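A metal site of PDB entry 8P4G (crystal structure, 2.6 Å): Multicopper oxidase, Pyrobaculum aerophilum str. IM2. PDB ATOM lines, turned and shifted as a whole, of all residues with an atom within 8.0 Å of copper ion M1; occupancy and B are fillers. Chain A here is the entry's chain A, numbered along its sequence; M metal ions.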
ATOM      1  N   HIS A  55     -25.881  -2.831 -23.266  1.00  0.00           N
ATOM      2  CA  HIS A  55     -25.964  -3.367 -21.926  1.00  0.00           C
ATOM      3  C   HIS A  55     -26.179  -2.227 -20.950  1.00  0.00           C
ATOM      4  O   HIS A  55     -25.403  -1.271 -20.931  1.00  0.00           O
ATOM      5  CB  HIS A  55     -24.708  -4.153 -21.551  1.00  0.00           C
ATOM      6  CG  HIS A  55     -24.669  -4.547 -20.112  1.00  0.00           C
ATOM      7  ND1 HIS A  55     -25.771  -5.034 -19.431  1.00  0.00           N
ATOM      8  CD2 HIS A  55     -23.664  -4.495 -19.196  1.00  0.00           C
ATOM      9  CE1 HIS A  55     -25.444  -5.282 -18.184  1.00  0.00           C
ATOM     10  NE2 HIS A  55     -24.165  -4.958 -18.011  1.00  0.00           N
ATOM     11  N   TRP A  56     -27.237  -2.322 -20.149  1.00  0.00           N
ATOM     12  CA  TRP A  56     -27.491  -1.361 -19.076  1.00  0.00           C
ATOM     13  C   TRP A  56     -26.706  -1.837 -17.863  1.00  0.00           C
ATOM     14  O   TRP A  56     -27.182  -2.641 -17.065  1.00  0.00           O
ATOM     15  CB  TRP A  56     -28.984  -1.259 -18.776  1.00  0.00           C
ATOM     16  CG  TRP A  56     -29.798  -0.782 -19.944  1.00  0.00           C
ATOM     17  CD1 TRP A  56     -30.364  -1.551 -20.915  1.00  0.00           C
ATOM     18  CD2 TRP A  56     -30.142   0.569 -20.250  1.00  0.00           C
ATOM     19  NE1 TRP A  56     -31.040  -0.761 -21.822  1.00  0.00           N
ATOM     20  CE2 TRP A  56     -30.915   0.547 -21.422  1.00  0.00           C
ATOM     21  CE3 TRP A  56     -29.872   1.803 -19.642  1.00  0.00           C
ATOM     22  CZ2 TRP A  56     -31.426   1.713 -22.012  1.00  0.00           C
ATOM     23  CZ3 TRP A  56     -30.379   2.953 -20.230  1.00  0.00           C
ATOM     24  CH2 TRP A  56     -31.142   2.898 -21.401  1.00  0.00           C
ATOM     25  N   HIS A  57     -25.475  -1.343 -17.736  1.00  0.00           N
ATOM     26  CA  HIS A  57     -24.549  -1.842 -16.738  1.00  0.00           C
ATOM     27  C   HIS A  57     -25.091  -1.631 -15.337  1.00  0.00           C
ATOM     28  O   HIS A  57     -25.311  -0.484 -14.909  1.00  0.00           O
ATOM     29  CB  HIS A  57     -23.190  -1.162 -16.901  1.00  0.00           C
ATOM     30  CG  HIS A  57     -22.136  -1.678 -15.977  1.00  0.00           C
ATOM     31  ND1 HIS A  57     -21.020  -2.350 -16.434  1.00  0.00           N
ATOM     32  CD2 HIS A  57     -22.018  -1.635 -14.631  1.00  0.00           C
ATOM     33  CE1 HIS A  57     -20.258  -2.687 -15.401  1.00  0.00           C
ATOM     34  NE2 HIS A  57     -20.846  -2.268 -14.298  1.00  0.00           N
ATOM     35  N   GLY A  58     -25.314  -2.724 -14.615  1.00  0.00           N
ATOM     36  CA  GLY A  58     -25.762  -2.662 -13.230  1.00  0.00           C
ATOM     37  C   GLY A  58     -27.258  -2.585 -13.026  1.00  0.00           C
ATOM     38  O   GLY A  58     -27.684  -2.370 -11.877  1.00  0.00           O
ATOM     39  N   LEU A  93     -24.059   2.822 -16.302  1.00  0.00           N
ATOM     40  CA  LEU A  93     -23.506   2.955 -17.640  1.00  0.00           C
ATOM     41  C   LEU A  93     -24.440   2.321 -18.656  1.00  0.00           C
ATOM     42  O   LEU A  93     -25.321   1.526 -18.331  1.00  0.00           O
ATOM     43  CB  LEU A  93     -22.127   2.281 -17.755  1.00  0.00           C
ATOM     44  CG  LEU A  93     -21.101   2.388 -16.625  1.00  0.00           C
ATOM     45  CD1 LEU A  93     -20.007   1.359 -16.836  1.00  0.00           C
ATOM     46  CD2 LEU A  93     -20.514   3.785 -16.577  1.00  0.00           C
ATOM     47  N   TYR A  94     -24.231   2.699 -19.922  1.00  0.00           N
ATOM     48  CA  TYR A  94     -24.762   1.960 -21.055  1.00  0.00           C
ATOM     49  C   TYR A  94     -23.696   1.914 -22.144  1.00  0.00           C
ATOM     50  O   TYR A  94     -23.176   2.958 -22.552  1.00  0.00           O
ATOM     51  CB  TYR A  94     -26.076   2.554 -21.580  1.00  0.00           C
ATOM     52  CG  TYR A  94     -26.007   3.961 -22.145  1.00  0.00           C
ATOM     53  CD1 TYR A  94     -26.112   5.075 -21.318  1.00  0.00           C
ATOM     54  CD2 TYR A  94     -25.862   4.176 -23.514  1.00  0.00           C
ATOM     55  CE1 TYR A  94     -26.064   6.360 -21.829  1.00  0.00           C
ATOM     56  CE2 TYR A  94     -25.815   5.460 -24.038  1.00  0.00           C
ATOM     57  CZ  TYR A  94     -25.920   6.539 -23.187  1.00  0.00           C
ATOM     58  OH  TYR A  94     -25.866   7.813 -23.704  1.00  0.00           O
ATOM     59  N   HIS A  95     -23.360   0.708 -22.590  1.00  0.00           N
ATOM     60  CA  HIS A  95     -22.239   0.491 -23.477  1.00  0.00           C
ATOM     61  C   HIS A  95     -22.496  -0.770 -24.283  1.00  0.00           C
ATOM     62  O   HIS A  95     -23.413  -1.545 -23.964  1.00  0.00           O
ATOM     63  CB  HIS A  95     -20.922   0.394 -22.696  1.00  0.00           C
ATOM     64  CG  HIS A  95     -20.857  -0.761 -21.750  1.00  0.00           C
ATOM     65  ND1 HIS A  95     -20.660  -2.058 -22.170  1.00  0.00           N
ATOM     66  CD2 HIS A  95     -20.933  -0.813 -20.393  1.00  0.00           C
ATOM     67  CE1 HIS A  95     -20.644  -2.866 -21.121  1.00  0.00           C
ATOM     68  NE2 HIS A  95     -20.800  -2.135 -20.037  1.00  0.00           N
ATOM     69  N   PRO A  96     -21.735  -1.013 -25.351  1.00  0.00           N
ATOM     70  CA  PRO A  96     -21.998  -2.199 -26.177  1.00  0.00           C
ATOM     71  C   PRO A  96     -21.670  -3.479 -25.434  1.00  0.00           C
ATOM     72  O   PRO A  96     -20.923  -3.500 -24.455  1.00  0.00           O
ATOM     73  CB  PRO A  96     -21.064  -2.006 -27.381  1.00  0.00           C
ATOM     74  CG  PRO A  96     -20.663  -0.591 -27.362  1.00  0.00           C
ATOM     75  CD  PRO A  96     -20.655  -0.190 -25.930  1.00  0.00           C
ATOM     76  N   HIS A  97     -22.244  -4.569 -25.936  1.00  0.00           N
ATOM     77  CA  HIS A  97     -21.883  -5.877 -25.401  1.00  0.00           C
ATOM     78  C   HIS A  97     -21.938  -7.022 -26.404  1.00  0.00           C
ATOM     79  O   HIS A  97     -22.343  -8.126 -26.029  1.00  0.00           O
ATOM     80  CB  HIS A  97     -22.792  -6.202 -24.216  1.00  0.00           C
ATOM     81  CG  HIS A  97     -22.111  -6.948 -23.106  1.00  0.00           C
ATOM     82  ND1 HIS A  97     -21.651  -8.234 -23.265  1.00  0.00           N
ATOM     83  CD2 HIS A  97     -21.807  -6.588 -21.844  1.00  0.00           C
ATOM     84  CE1 HIS A  97     -21.090  -8.640 -22.138  1.00  0.00           C
ATOM     85  NE2 HIS A  97     -21.165  -7.659 -21.253  1.00  0.00           N
ATOM     86  N   THR A 102     -16.796  -5.911 -28.370  1.00  0.00           N
ATOM     87  CA  THR A 102     -17.179  -4.879 -27.413  1.00  0.00           C
ATOM     88  C   THR A 102     -16.073  -3.862 -27.206  1.00  0.00           C
ATOM     89  O   THR A 102     -16.343  -2.655 -27.142  1.00  0.00           O
ATOM     90  CB  THR A 102     -17.562  -5.534 -26.080  1.00  0.00           C
ATOM     91  OG1 THR A 102     -18.716  -6.364 -26.257  1.00  0.00           O
ATOM     92  CG2 THR A 102     -17.857  -4.478 -25.034  1.00  0.00           C
ATOM     93  N   PHE A 106     -16.637   0.084 -27.646  1.00  0.00           N
ATOM     94  CA  PHE A 106     -16.497   0.875 -26.421  1.00  0.00           C
ATOM     95  C   PHE A 106     -15.391   1.912 -26.572  1.00  0.00           C
ATOM     96  O   PHE A 106     -15.614   3.106 -26.340  1.00  0.00           O
ATOM     97  CB  PHE A 106     -16.199  -0.082 -25.255  1.00  0.00           C
ATOM     98  CG  PHE A 106     -16.343   0.526 -23.892  1.00  0.00           C
ATOM     99  CD1 PHE A 106     -17.389   0.141 -23.068  1.00  0.00           C
ATOM    100  CD2 PHE A 106     -15.416   1.449 -23.412  1.00  0.00           C
ATOM    101  CE1 PHE A 106     -17.525   0.666 -21.804  1.00  0.00           C
ATOM    102  CE2 PHE A 106     -15.557   1.990 -22.150  1.00  0.00           C
ATOM    103  CZ  PHE A 106     -16.607   1.597 -21.346  1.00  0.00           C
ATOM    104  N   LEU A 111     -20.106   4.908 -25.349  1.00  0.00           N
ATOM    105  CA  LEU A 111     -20.216   4.834 -23.888  1.00  0.00           C
ATOM    106  C   LEU A 111     -20.969   6.059 -23.394  1.00  0.00           C
ATOM    107  O   LEU A 111     -20.666   7.181 -23.805  1.00  0.00           O
ATOM    108  CB  LEU A 111     -18.832   4.766 -23.236  1.00  0.00           C
ATOM    109  CG  LEU A 111     -18.880   4.882 -21.703  1.00  0.00           C
ATOM    110  CD1 LEU A 111     -19.624   3.691 -21.100  1.00  0.00           C
ATOM    111  CD2 LEU A 111     -17.479   5.013 -21.112  1.00  0.00           C
ATOM    112  N   PRO A 231     -11.844  -0.410 -14.318  1.00  0.00           N
ATOM    113  CA  PRO A 231     -12.808  -0.180 -15.404  1.00  0.00           C
ATOM    114  C   PRO A 231     -14.229  -0.538 -15.007  1.00  0.00           C
ATOM    115  O   PRO A 231     -14.485  -1.608 -14.454  1.00  0.00           O
ATOM    116  CB  PRO A 231     -12.291  -1.082 -16.525  1.00  0.00           C
ATOM    117  CG  PRO A 231     -10.826  -1.101 -16.317  1.00  0.00           C
ATOM    118  CD  PRO A 231     -10.617  -1.066 -14.814  1.00  0.00           C
ATOM    119  N   ALA A 232     -15.152   0.390 -15.271  1.00  0.00           N
ATOM    120  CA  ALA A 232     -16.592   0.322 -15.039  1.00  0.00           C
ATOM    121  C   ALA A 232     -16.984   0.500 -13.576  1.00  0.00           C
ATOM    122  O   ALA A 232     -18.182   0.414 -13.263  1.00  0.00           O
ATOM    123  CB  ALA A 232     -17.222  -0.977 -15.561  1.00  0.00           C
ATOM    124  N   GLU A 233     -16.039   0.740 -12.671  1.00  0.00           N
ATOM    125  CA  GLU A 233     -16.400   1.070 -11.301  1.00  0.00           C
ATOM    126  C   GLU A 233     -16.833   2.528 -11.210  1.00  0.00           C
ATOM    127  O   GLU A 233     -16.391   3.384 -11.987  1.00  0.00           O
ATOM    128  CB  GLU A 233     -15.239   0.815 -10.344  1.00  0.00           C
ATOM    129  CG  GLU A 233     -14.999  -0.647 -10.021  1.00  0.00           C
ATOM    130  CD  GLU A 233     -13.998  -0.841  -8.898  1.00  0.00           C
ATOM    131  OE1 GLU A 233     -12.894  -0.257  -8.975  1.00  0.00           O
ATOM    132  OE2 GLU A 233     -14.308  -1.565  -7.936  1.00  0.00           O
ATOM    133  N   ARG A 234     -17.699   2.821 -10.244  1.00  0.00           N
ATOM    134  CA  ARG A 234     -18.174   4.169  -9.990  1.00  0.00           C
ATOM    135  C   ARG A 234     -17.976   4.499  -8.517  1.00  0.00           C
ATOM    136  O   ARG A 234     -18.167   3.646  -7.654  1.00  0.00           O
ATOM    137  CB  ARG A 234     -19.666   4.338 -10.357  1.00  0.00           C
ATOM    138  CG  ARG A 234     -19.958   4.280 -11.859  1.00  0.00           C
ATOM    139  CD  ARG A 234     -20.131   2.852 -12.337  1.00  0.00           C
ATOM    140  NE  ARG A 234     -21.431   2.299 -11.933  1.00  0.00           N
ATOM    141  CZ  ARG A 234     -21.676   1.001 -11.826  1.00  0.00           C
ATOM    142  NH1 ARG A 234     -20.722   0.117 -12.073  1.00  0.00           N
ATOM    143  NH2 ARG A 234     -22.885   0.585 -11.462  1.00  0.00           N
ATOM    144  N   HIS A 357     -17.274  -8.495 -12.990  1.00  0.00           N
ATOM    145  CA  HIS A 357     -18.587  -7.862 -12.970  1.00  0.00           C
ATOM    146  C   HIS A 357     -19.655  -8.904 -13.278  1.00  0.00           C
ATOM    147  O   HIS A 357     -19.491  -9.723 -14.184  1.00  0.00           O
ATOM    148  CB  HIS A 357     -18.658  -6.713 -13.986  1.00  0.00           C
ATOM    149  CG  HIS A 357     -20.034  -6.164 -14.174  1.00  0.00           C
ATOM    150  ND1 HIS A 357     -20.873  -5.866 -13.132  1.00  0.00           N
ATOM    151  CD2 HIS A 357     -20.725  -5.879 -15.308  1.00  0.00           C
ATOM    152  CE1 HIS A 357     -22.018  -5.402 -13.603  1.00  0.00           C
ATOM    153  NE2 HIS A 357     -21.949  -5.403 -14.926  1.00  0.00           N
ATOM    154  N   HIS A 359     -23.750  -9.546 -14.116  1.00  0.00           N
ATOM    155  CA  HIS A 359     -24.994  -8.973 -14.601  1.00  0.00           C
ATOM    156  C   HIS A 359     -26.178  -9.392 -13.720  1.00  0.00           C
ATOM    157  O   HIS A 359     -26.154 -10.418 -13.031  1.00  0.00           O
ATOM    158  CB  HIS A 359     -25.281  -9.404 -16.044  1.00  0.00           C
ATOM    159  CG  HIS A 359     -24.328  -8.840 -17.046  1.00  0.00           C
ATOM    160  ND1 HIS A 359     -24.742  -8.394 -18.288  1.00  0.00           N
ATOM    161  CD2 HIS A 359     -22.987  -8.675 -17.008  1.00  0.00           C
ATOM    162  CE1 HIS A 359     -23.692  -7.964 -18.959  1.00  0.00           C
ATOM    163  NE2 HIS A 359     -22.614  -8.123 -18.217  1.00  0.00           N
ATOM    164  N   ASP A 394     -21.370  -3.743  -8.128  1.00  0.00           N
ATOM    165  CA  ASP A 394     -21.528  -4.688  -9.232  1.00  0.00           C
ATOM    166  C   ASP A 394     -20.235  -4.951  -9.987  1.00  0.00           C
ATOM    167  O   ASP A 394     -20.217  -5.827 -10.855  1.00  0.00           O
ATOM    168  CB  ASP A 394     -22.597  -4.205 -10.223  1.00  0.00           C
ATOM    169  CG  ASP A 394     -22.277  -2.858 -10.854  1.00  0.00           C
ATOM    170  OD1 ASP A 394     -21.203  -2.718 -11.475  1.00  0.00           O
ATOM    171  OD2 ASP A 394     -23.118  -1.938 -10.733  1.00  0.00           O
ATOM    172  N   THR A 395     -19.150  -4.242  -9.688  1.00  0.00           N
ATOM    173  CA  THR A 395     -17.846  -4.463 -10.304  1.00  0.00           C
ATOM    174  C   THR A 395     -16.786  -4.313  -9.223  1.00  0.00           C
ATOM    175  O   THR A 395     -16.591  -3.212  -8.698  1.00  0.00           O
ATOM    176  CB  THR A 395     -17.591  -3.484 -11.454  1.00  0.00           C
ATOM    177  OG1 THR A 395     -18.670  -3.558 -12.391  1.00  0.00           O
ATOM    178  CG2 THR A 395     -16.278  -3.816 -12.155  1.00  0.00           C
ATOM    179  N   HIS A 422     -18.207 -11.774 -16.070  1.00  0.00           N
ATOM    180  CA  HIS A 422     -16.997 -11.588 -16.855  1.00  0.00           C
ATOM    181  C   HIS A 422     -16.112 -10.545 -16.190  1.00  0.00           C
ATOM    182  O   HIS A 422     -16.544  -9.813 -15.297  1.00  0.00           O
ATOM    183  CB  HIS A 422     -17.324 -11.171 -18.280  1.00  0.00           C
ATOM    184  CG  HIS A 422     -18.018  -9.845 -18.376  1.00  0.00           C
ATOM    185  ND1 HIS A 422     -17.337  -8.645 -18.433  1.00  0.00           N
ATOM    186  CD2 HIS A 422     -19.344  -9.531 -18.413  1.00  0.00           C
ATOM    187  CE1 HIS A 422     -18.205  -7.654 -18.509  1.00  0.00           C
ATOM    188  NE2 HIS A 422     -19.423  -8.160 -18.500  1.00  0.00           N
ATOM    189  N   HIS A 424     -14.204  -7.018 -16.552  1.00  0.00           N
ATOM    190  CA  HIS A 424     -14.502  -5.801 -17.298  1.00  0.00           C
ATOM    191  C   HIS A 424     -13.265  -5.183 -17.923  1.00  0.00           C
ATOM    192  O   HIS A 424     -13.334  -4.070 -18.452  1.00  0.00           O
ATOM    193  CB  HIS A 424     -15.215  -4.787 -16.406  1.00  0.00           C
ATOM    194  CG  HIS A 424     -16.401  -4.148 -17.058  1.00  0.00           C
ATOM    195  ND1 HIS A 424     -16.296  -3.219 -18.063  1.00  0.00           N
ATOM    196  CD2 HIS A 424     -17.724  -4.328 -16.848  1.00  0.00           C
ATOM    197  CE1 HIS A 424     -17.504  -2.852 -18.457  1.00  0.00           C
ATOM    198  NE2 HIS A 424     -18.389  -3.510 -17.730  1.00  0.00           N
ATOM    199  N   LEU A 426     -11.778  -5.043 -21.034  1.00  0.00           N
ATOM    200  CA  LEU A 426     -12.471  -5.330 -22.291  1.00  0.00           C
ATOM    201  C   LEU A 426     -11.646  -6.208 -23.219  1.00  0.00           C
ATOM    202  O   LEU A 426     -12.204  -6.947 -24.036  1.00  0.00           O
ATOM    203  CB  LEU A 426     -12.860  -4.021 -22.974  1.00  0.00           C
ATOM    204  CG  LEU A 426     -13.821  -3.182 -22.146  1.00  0.00           C
ATOM    205  CD1 LEU A 426     -14.331  -2.009 -22.949  1.00  0.00           C
ATOM    206  CD2 LEU A 426     -14.981  -4.037 -21.636  1.00  0.00           C
ATOM    207  N   GLU A 429     -12.412  -9.652 -21.770  1.00  0.00           N
ATOM    208  CA  GLU A 429     -13.766 -10.072 -22.099  1.00  0.00           C
ATOM    209  C   GLU A 429     -13.891 -10.466 -23.565  1.00  0.00           C
ATOM    210  O   GLU A 429     -14.452 -11.518 -23.893  1.00  0.00           O
ATOM    211  CB  GLU A 429     -14.762  -8.966 -21.768  1.00  0.00           C
ATOM    212  CG  GLU A 429     -16.200  -9.359 -22.057  1.00  0.00           C
ATOM    213  CD  GLU A 429     -17.122  -8.167 -22.130  1.00  0.00           C
ATOM    214  OE1 GLU A 429     -16.861  -7.175 -21.416  1.00  0.00           O
ATOM    215  OE2 GLU A 429     -18.099  -8.221 -22.898  1.00  0.00           O
HETATM  216 CU    CU M   1     -20.344  -2.819 -18.159  1.00  0.00          CU
HETATM  217 CU    CU M   2     -22.651  -5.367 -16.359  1.00  0.00          CU
HETATM  218 CU    CU M   3     -21.021  -6.926 -18.941  1.00  0.00          CU
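A ring nitrogen (NE2) of His 57 sits at hydrogen-bond distance from the guanidinium group of Arg 234. A ring nitrogen (NE2) of His 57 sits at hydrogen-bond distance from the side-chain carboxylate (OD1) of Asp 394, at 2.9 Å. The backbone NH of His 57 lies within hydrogen-bond range of the backbone carbonyl oxygen of Leu 93 (2.9 Å). A ring nitrogen (NE2) of His 57 is in hydrogen-bond range of the side-chain hydroxyl (OG1) of Thr 395 (3.2 Å). The backbone NH (N) of His 55 sits at hydrogen-bond distance from the backbone carbonyl oxygen (O) of His 95 (2.9 Å). NE2 of His 55 lies close to ND1 of His 359, 3.5 Å away. A ring nitrogen (NE2) of His 57 lies close to a ring nitrogen (NE2) of His 357.
Residues that only touch copper ion M1: His 55. Four residues have an atom within 4 Å of copper ion M1: His 55, His 57, His 95 and His 424. Along chain A the residues within 4 Å of copper ion M1 span positions 55 to 424. The nearest printed residue that does not touch copper ion M1 is His 357 (4.2 Å).
Copper ion M1 is bound by ND1 of His 57, 1.9 Å away. NE2 of His 95 binds copper ion M1. Copper ion M1 is bound by NE2 of His 424 (2.1 Å).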
